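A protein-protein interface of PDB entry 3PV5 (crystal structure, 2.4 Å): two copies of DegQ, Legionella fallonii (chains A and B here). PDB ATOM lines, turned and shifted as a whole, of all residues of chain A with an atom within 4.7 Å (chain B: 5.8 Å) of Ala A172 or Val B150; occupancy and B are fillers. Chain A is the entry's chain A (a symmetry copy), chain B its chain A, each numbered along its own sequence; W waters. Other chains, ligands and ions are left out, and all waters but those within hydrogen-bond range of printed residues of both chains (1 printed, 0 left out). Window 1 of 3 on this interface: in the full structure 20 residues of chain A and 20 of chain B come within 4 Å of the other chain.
The backbone carbonyl oxygen (O) of Ser B178 sits at hydrogen-bond distance from the backbone NH (N) of Ala A172, 3.0 Å away.
The side-chain carboxylate (OD2) of Asp B197 lies within hydrogen-bond range of the side-chain hydroxyl (OG1) of Thr A173.
The side-chain carboxylate of Asp B197 sits at hydrogen-bond distance from the backbone NH of Phe A174 (2.8 Å).
OD1 of Asp B197 is in hydrogen-bond range of N of Ile B176 (2.9 Å).
N of Val B177 is in hydrogen-bond range of O of Asp B152 (2.9 Å).
The backbone NH (N) of Gly B151 is in hydrogen-bond range of the backbone carbonyl oxygen (O) of Val B177, at 3.0 Å.
OD2 of Asp B152 is in hydrogen-bond range of N of Glu B149 (2.9 Å).
OG1 of Thr B196 sits close to O of Ile B176.
The backbone carbonyl oxygen of Thr A173 sits at hydrogen-bond distance from the backbone NH of Ala A156 (2.9 Å).
Ala A22 touches Glu B149.
Val B150 touches Ala A22 (O to CA, 3.4 Å).
Ala A22 touches Gly B151.
Ala A22 touches Asp B152 (CB to OD1, 3.7 Å).
Met A29 touches Val B150.
Ser B178 touches Ser A171 (O to CA, 3.5 Å).
Val B150 touches Ala A172.
CD1 of Ile B176 touches O of Ala A172, at 3.9 Å.
Phe A174 touches Ile B176.
Ile A200 touches Asp B197 (CG2 to CB, 3.9 Å).
Ala A172 touches just these residues of chain B: Val B150 (3.9 Å), Ile B176 (3.9 Å) and Ser B178 (2.8 Å).
Of chain A, only Ala A22 (3.4 Å), Met A29 (3.96 Å) and Ala A172 (3.9 Å) come within 4 Å of Val B150.
Printed residues of chain A within 4 Å of Ser B178: Ser A171 (3.5 Å) and Ala A172 (2.8 Å).
Of the printed residues of chain A, Asp B197 touches Thr A173, Phe A174 and Ile A200.
The nearest residue of chain B that does not touch Ala A172 is Asp B197 (4.6 Å).
The nearest residue of chain A that does not touch Val B150 is Leu A25 (4.2 Å).
Of the 12 printed residues of chain B, 7 touch a printed residue of chain A.
Hydrophobic or aromatic side chains of chain B that line the printed part of chain A: Val B150 and Ile B176.
Of the 12 printed residues of chain A, 7 touch a printed residue of chain B.
Hydrophobic or aromatic side chains of chain A that line the printed part of chain B: Ala A22, Met A29, Ala A172, Phe A174 and Ile A200.
Among the printed residues, 13 pairs touch across the chains.
Among the printed residues, no Asp or Glu carboxylate lies within 4 Å of a Lys or Arg side-chain nitrogen of the other chain.
No position is printed for both chains.
Of the 13 pairs that touch across the chains among the printed residues, none has its exchanged pair printed and touching as well.
Water W1 lies within hydrogen-bond range of O of Ala A22 (2.8 Å) and O of Val B150 (2.9 Å).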
ATOM      1  N   ALA A  22     -10.874  30.443 -30.336  1.00  0.00           N
ATOM      2  CA  ALA A  22      -9.458  30.778 -30.360  1.00  0.00           C
ATOM      3  C   ALA A  22      -9.151  32.138 -30.981  1.00  0.00           C
ATOM      4  O   ALA A  22      -8.292  32.840 -30.473  1.00  0.00           O
ATOM      5  CB  ALA A  22      -8.626  29.694 -31.028  1.00  0.00           C
ATOM      6  N   LEU A  25     -10.140  35.000 -28.488  1.00  0.00           N
ATOM      7  CA  LEU A  25      -9.386  34.996 -27.233  1.00  0.00           C
ATOM      8  C   LEU A  25      -7.917  35.423 -27.421  1.00  0.00           C
ATOM      9  O   LEU A  25      -7.308  36.043 -26.550  1.00  0.00           O
ATOM     10  CB  LEU A  25      -9.452  33.620 -26.547  1.00  0.00           C
ATOM     11  CG  LEU A  25     -10.843  33.108 -26.082  1.00  0.00           C
ATOM     12  CD1 LEU A  25     -10.751  31.831 -25.196  1.00  0.00           C
ATOM     13  CD2 LEU A  25     -11.616  34.250 -25.355  1.00  0.00           C
ATOM     14  N   MET A  29      -6.608  38.216 -24.799  1.00  0.00           N
ATOM     15  CA  MET A  29      -5.799  37.688 -23.735  1.00  0.00           C
ATOM     16  C   MET A  29      -4.748  38.682 -23.119  1.00  0.00           C
ATOM     17  O   MET A  29      -4.522  38.688 -21.926  1.00  0.00           O
ATOM     18  CB  MET A  29      -5.117  36.415 -24.294  1.00  0.00           C
ATOM     19  CG  MET A  29      -4.797  35.377 -23.294  1.00  0.00           C
ATOM     20  SD  MET A  29      -6.212  34.535 -22.430  1.00  0.00           S
ATOM     21  CE  MET A  29      -7.007  33.610 -23.707  1.00  0.00           C
ATOM     22  N   VAL A 155     -16.963  33.259 -22.013  1.00  0.00           N
ATOM     23  CA  VAL A 155     -15.693  32.666 -21.602  1.00  0.00           C
ATOM     24  C   VAL A 155     -15.247  33.462 -20.449  1.00  0.00           C
ATOM     25  O   VAL A 155     -15.327  34.683 -20.524  1.00  0.00           O
ATOM     26  CB  VAL A 155     -14.621  32.716 -22.754  1.00  0.00           C
ATOM     27  CG1 VAL A 155     -13.209  32.260 -22.240  1.00  0.00           C
ATOM     28  CG2 VAL A 155     -15.090  31.881 -23.940  1.00  0.00           C
ATOM     29  N   ALA A 156     -14.858  32.774 -19.358  1.00  0.00           N
ATOM     30  CA  ALA A 156     -14.221  33.362 -18.206  1.00  0.00           C
ATOM     31  C   ALA A 156     -12.723  33.142 -18.290  1.00  0.00           C
ATOM     32  O   ALA A 156     -12.271  31.998 -18.376  1.00  0.00           O
ATOM     33  CB  ALA A 156     -14.788  32.763 -16.797  1.00  0.00           C
ATOM     34  N   ILE A 157     -11.952  34.235 -18.211  1.00  0.00           N
ATOM     35  CA  ILE A 157     -10.488  34.207 -18.373  1.00  0.00           C
ATOM     36  C   ILE A 157      -9.900  34.688 -17.105  1.00  0.00           C
ATOM     37  O   ILE A 157     -10.133  35.861 -16.679  1.00  0.00           O
ATOM     38  CB  ILE A 157      -9.998  35.101 -19.483  1.00  0.00           C
ATOM     39  CG1 ILE A 157     -10.547  34.661 -20.828  1.00  0.00           C
ATOM     40  CG2 ILE A 157      -8.434  35.099 -19.595  1.00  0.00           C
ATOM     41  CD1 ILE A 157     -10.919  35.803 -21.756  1.00  0.00           C
ATOM     42  N   GLN A 170      -3.198  32.945 -18.729  1.00  0.00           N
ATOM     43  CA  GLN A 170      -4.413  33.002 -17.954  1.00  0.00           C
ATOM     44  C   GLN A 170      -5.360  31.921 -18.442  1.00  0.00           C
ATOM     45  O   GLN A 170      -5.654  31.861 -19.626  1.00  0.00           O
ATOM     46  CB  GLN A 170      -5.013  34.389 -18.081  1.00  0.00           C
ATOM     47  CG  GLN A 170      -5.449  34.911 -16.753  1.00  0.00           C
ATOM     48  CD  GLN A 170      -4.308  35.456 -16.027  1.00  0.00           C
ATOM     49  OE1 GLN A 170      -3.464  36.065 -16.657  1.00  0.00           O
ATOM     50  NE2 GLN A 170      -4.213  35.215 -14.732  1.00  0.00           N
ATOM     51  N   SER A 171      -5.808  31.045 -17.547  1.00  0.00           N
ATOM     52  CA  SER A 171      -6.722  29.968 -17.960  1.00  0.00           C
ATOM     53  C   SER A 171      -8.032  30.504 -18.494  1.00  0.00           C
ATOM     54  O   SER A 171      -8.602  31.456 -17.936  1.00  0.00           O
ATOM     55  CB  SER A 171      -7.055  29.030 -16.817  1.00  0.00           C
ATOM     56  OG  SER A 171      -5.894  28.345 -16.356  1.00  0.00           O
ATOM     57  N   ALA A 172      -8.520  29.877 -19.568  1.00  0.00           N
ATOM     58  CA  ALA A 172      -9.834  30.167 -20.117  1.00  0.00           C
ATOM     59  C   ALA A 172     -10.846  28.993 -19.897  1.00  0.00           C
ATOM     60  O   ALA A 172     -10.504  27.829 -19.989  1.00  0.00           O
ATOM     61  CB  ALA A 172      -9.693  30.481 -21.556  1.00  0.00           C
ATOM     62  N   THR A 173     -12.109  29.324 -19.611  1.00  0.00           N
ATOM     63  CA  THR A 173     -13.157  28.327 -19.474  1.00  0.00           C
ATOM     64  C   THR A 173     -14.457  28.777 -20.095  1.00  0.00           C
ATOM     65  O   THR A 173     -14.775  29.945 -20.005  1.00  0.00           O
ATOM     66  CB  THR A 173     -13.454  28.025 -18.020  1.00  0.00           C
ATOM     67  OG1 THR A 173     -14.362  26.949 -18.019  1.00  0.00           O
ATOM     68  CG2 THR A 173     -14.078  29.230 -17.239  1.00  0.00           C
ATOM     69  N   PHE A 174     -15.200  27.838 -20.696  1.00  0.00           N
ATOM     70  CA  PHE A 174     -16.333  28.153 -21.608  1.00  0.00           C
ATOM     71  C   PHE A 174     -17.697  27.655 -21.077  1.00  0.00           C
ATOM     72  O   PHE A 174     -17.803  26.603 -20.396  1.00  0.00           O
ATOM     73  CB  PHE A 174     -16.056  27.586 -23.001  1.00  0.00           C
ATOM     74  CG  PHE A 174     -17.250  27.569 -23.970  1.00  0.00           C
ATOM     75  CD1 PHE A 174     -17.421  28.570 -24.902  1.00  0.00           C
ATOM     76  CD2 PHE A 174     -18.158  26.508 -23.981  1.00  0.00           C
ATOM     77  CE1 PHE A 174     -18.477  28.546 -25.854  1.00  0.00           C
ATOM     78  CE2 PHE A 174     -19.222  26.472 -24.915  1.00  0.00           C
ATOM     79  CZ  PHE A 174     -19.383  27.521 -25.835  1.00  0.00           C
ATOM     80  N   ILE A 200     -13.716  27.181 -13.268  1.00  0.00           N
ATOM     81  CA  ILE A 200     -12.735  26.160 -13.037  1.00  0.00           C
ATOM     82  C   ILE A 200     -12.087  26.383 -11.703  1.00  0.00           C
ATOM     83  O   ILE A 200     -11.913  27.527 -11.288  1.00  0.00           O
ATOM     84  CB  ILE A 200     -11.700  26.023 -14.206  1.00  0.00           C
ATOM     85  CG1 ILE A 200     -11.164  27.371 -14.654  1.00  0.00           C
ATOM     86  CG2 ILE A 200     -12.336  25.217 -15.403  1.00  0.00           C
ATOM     87  CD1 ILE A 200      -9.785  27.275 -15.475  1.00  0.00           C
ATOM     88  N   LEU B 148      -2.738  23.143 -31.610  1.00  0.00           N
ATOM     89  CA  LEU B 148      -3.816  23.498 -30.695  1.00  0.00           C
ATOM     90  C   LEU B 148      -3.766  24.902 -30.172  1.00  0.00           C
ATOM     91  O   LEU B 148      -2.695  25.379 -29.815  1.00  0.00           O
ATOM     92  CB  LEU B 148      -3.741  22.611 -29.470  1.00  0.00           C
ATOM     93  CG  LEU B 148      -4.419  21.262 -29.575  1.00  0.00           C
ATOM     94  CD1 LEU B 148      -4.184  20.552 -28.256  1.00  0.00           C
ATOM     95  CD2 LEU B 148      -5.971  21.404 -29.914  1.00  0.00           C
ATOM     96  N   GLU B 149      -4.932  25.533 -30.030  1.00  0.00           N
ATOM     97  CA  GLU B 149      -5.051  26.820 -29.359  1.00  0.00           C
ATOM     98  C   GLU B 149      -6.111  26.858 -28.274  1.00  0.00           C
ATOM     99  O   GLU B 149      -7.189  26.237 -28.378  1.00  0.00           O
ATOM    100  CB  GLU B 149      -5.392  27.905 -30.332  1.00  0.00           C
ATOM    101  CG  GLU B 149      -4.560  27.902 -31.592  1.00  0.00           C
ATOM    102  CD  GLU B 149      -4.694  29.202 -32.277  1.00  0.00           C
ATOM    103  OE1 GLU B 149      -5.396  29.283 -33.302  1.00  0.00           O
ATOM    104  OE2 GLU B 149      -4.163  30.173 -31.698  1.00  0.00           O
ATOM    105  N   VAL B 150      -5.799  27.653 -27.251  1.00  0.00           N
ATOM    106  CA  VAL B 150      -6.723  28.019 -26.190  1.00  0.00           C
ATOM    107  C   VAL B 150      -7.941  28.522 -26.872  1.00  0.00           C
ATOM    108  O   VAL B 150      -7.827  29.364 -27.754  1.00  0.00           O
ATOM    109  CB  VAL B 150      -6.133  29.091 -25.360  1.00  0.00           C
ATOM    110  CG1 VAL B 150      -7.215  29.717 -24.423  1.00  0.00           C
ATOM    111  CG2 VAL B 150      -4.991  28.488 -24.614  1.00  0.00           C
ATOM    112  N   GLY B 151      -9.081  27.917 -26.543  1.00  0.00           N
ATOM    113  CA  GLY B 151     -10.337  28.264 -27.213  1.00  0.00           C
ATOM    114  C   GLY B 151     -10.896  27.253 -28.182  1.00  0.00           C
ATOM    115  O   GLY B 151     -12.046  27.340 -28.527  1.00  0.00           O
ATOM    116  N   ASP B 152     -10.103  26.295 -28.637  1.00  0.00           N
ATOM    117  CA  ASP B 152     -10.609  25.243 -29.522  1.00  0.00           C
ATOM    118  C   ASP B 152     -11.497  24.307 -28.713  1.00  0.00           C
ATOM    119  O   ASP B 152     -11.234  23.988 -27.542  1.00  0.00           O
ATOM    120  CB  ASP B 152      -9.450  24.421 -30.101  1.00  0.00           C
ATOM    121  CG  ASP B 152      -8.594  25.198 -31.169  1.00  0.00           C
ATOM    122  OD1 ASP B 152      -9.085  26.100 -31.893  1.00  0.00           O
ATOM    123  OD2 ASP B 152      -7.402  24.849 -31.291  1.00  0.00           O
ATOM    124  N   ILE B 176     -13.485  23.423 -23.961  1.00  0.00           N
ATOM    125  CA  ILE B 176     -12.423  24.033 -24.755  1.00  0.00           C
ATOM    126  C   ILE B 176     -11.086  23.741 -24.144  1.00  0.00           C
ATOM    127  O   ILE B 176     -10.977  23.372 -22.968  1.00  0.00           O
ATOM    128  CB  ILE B 176     -12.631  25.508 -24.846  1.00  0.00           C
ATOM    129  CG1 ILE B 176     -12.209  26.159 -23.517  1.00  0.00           C
ATOM    130  CG2 ILE B 176     -14.056  25.764 -25.231  1.00  0.00           C
ATOM    131  CD1 ILE B 176     -12.336  27.607 -23.463  1.00  0.00           C
ATOM    132  N   VAL B 177     -10.041  23.866 -24.942  1.00  0.00           N
ATOM    133  CA  VAL B 177      -8.663  23.942 -24.383  1.00  0.00           C
ATOM    134  C   VAL B 177      -8.548  25.203 -23.509  1.00  0.00           C
ATOM    135  O   VAL B 177      -8.816  26.254 -24.011  1.00  0.00           O
ATOM    136  CB  VAL B 177      -7.638  24.072 -25.586  1.00  0.00           C
ATOM    137  CG1 VAL B 177      -6.161  24.232 -25.079  1.00  0.00           C
ATOM    138  CG2 VAL B 177      -7.783  22.874 -26.541  1.00  0.00           C
ATOM    139  N   SER B 178      -8.177  25.111 -22.230  1.00  0.00           N
ATOM    140  CA  SER B 178      -8.074  26.291 -21.341  1.00  0.00           C
ATOM    141  C   SER B 178      -6.676  26.887 -21.278  1.00  0.00           C
ATOM    142  O   SER B 178      -6.575  28.058 -20.942  1.00  0.00           O
ATOM    143  CB  SER B 178      -8.337  26.035 -19.824  1.00  0.00           C
ATOM    144  OG  SER B 178      -9.192  24.994 -19.570  1.00  0.00           O
ATOM    145  N   ALA B 179      -5.656  26.039 -21.360  1.00  0.00           N
ATOM    146  CA  ALA B 179      -4.247  26.472 -21.360  1.00  0.00           C
ATOM    147  C   ALA B 179      -3.330  25.409 -21.999  1.00  0.00           C
ATOM    148  O   ALA B 179      -3.512  24.220 -21.788  1.00  0.00           O
ATOM    149  CB  ALA B 179      -3.747  26.781 -19.933  1.00  0.00           C
ATOM    150  N   LEU B 180      -2.340  25.867 -22.753  1.00  0.00           N
ATOM    151  CA  LEU B 180      -1.387  24.989 -23.388  1.00  0.00           C
ATOM    152  C   LEU B 180      -0.299  24.562 -22.451  1.00  0.00           C
ATOM    153  O   LEU B 180      -0.009  25.217 -21.477  1.00  0.00           O
ATOM    154  CB  LEU B 180      -0.770  25.664 -24.591  1.00  0.00           C
ATOM    155  CG  LEU B 180      -1.756  26.062 -25.691  1.00  0.00           C
ATOM    156  CD1 LEU B 180      -0.949  26.716 -26.821  1.00  0.00           C
ATOM    157  CD2 LEU B 180      -2.585  24.922 -26.204  1.00  0.00           C
ATOM    158  N   THR B 196      -7.740  21.690 -20.120  1.00  0.00           N
ATOM    159  CA  THR B 196      -9.049  21.754 -20.706  1.00  0.00           C
ATOM    160  C   THR B 196     -10.058  22.086 -19.607  1.00  0.00           C
ATOM    161  O   THR B 196      -9.766  21.819 -18.454  1.00  0.00           O
ATOM    162  CB  THR B 196      -9.425  20.255 -21.071  1.00  0.00           C
ATOM    163  OG1 THR B 196     -10.535  20.154 -21.922  1.00  0.00           O
ATOM    164  CG2 THR B 196      -9.978  19.632 -19.921  1.00  0.00           C
ATOM    165  N   ASP B 197     -11.297  22.501 -19.953  1.00  0.00           N
ATOM    166  CA  ASP B 197     -12.450  22.395 -19.000  1.00  0.00           C
ATOM    167  C   ASP B 197     -13.462  21.258 -19.344  1.00  0.00           C
ATOM    168  O   ASP B 197     -14.620  21.328 -19.020  1.00  0.00           O
ATOM    169  CB  ASP B 197     -13.233  23.710 -18.833  1.00  0.00           C
ATOM    170  CG  ASP B 197     -13.880  24.139 -20.066  1.00  0.00           C
ATOM    171  OD1 ASP B 197     -13.882  23.398 -21.098  1.00  0.00           O
ATOM    172  OD2 ASP B 197     -14.340  25.278 -20.036  1.00  0.00           O
HETATM  173  O   HOH W   1      -6.514  31.750 -28.654  1.00  0.00           O
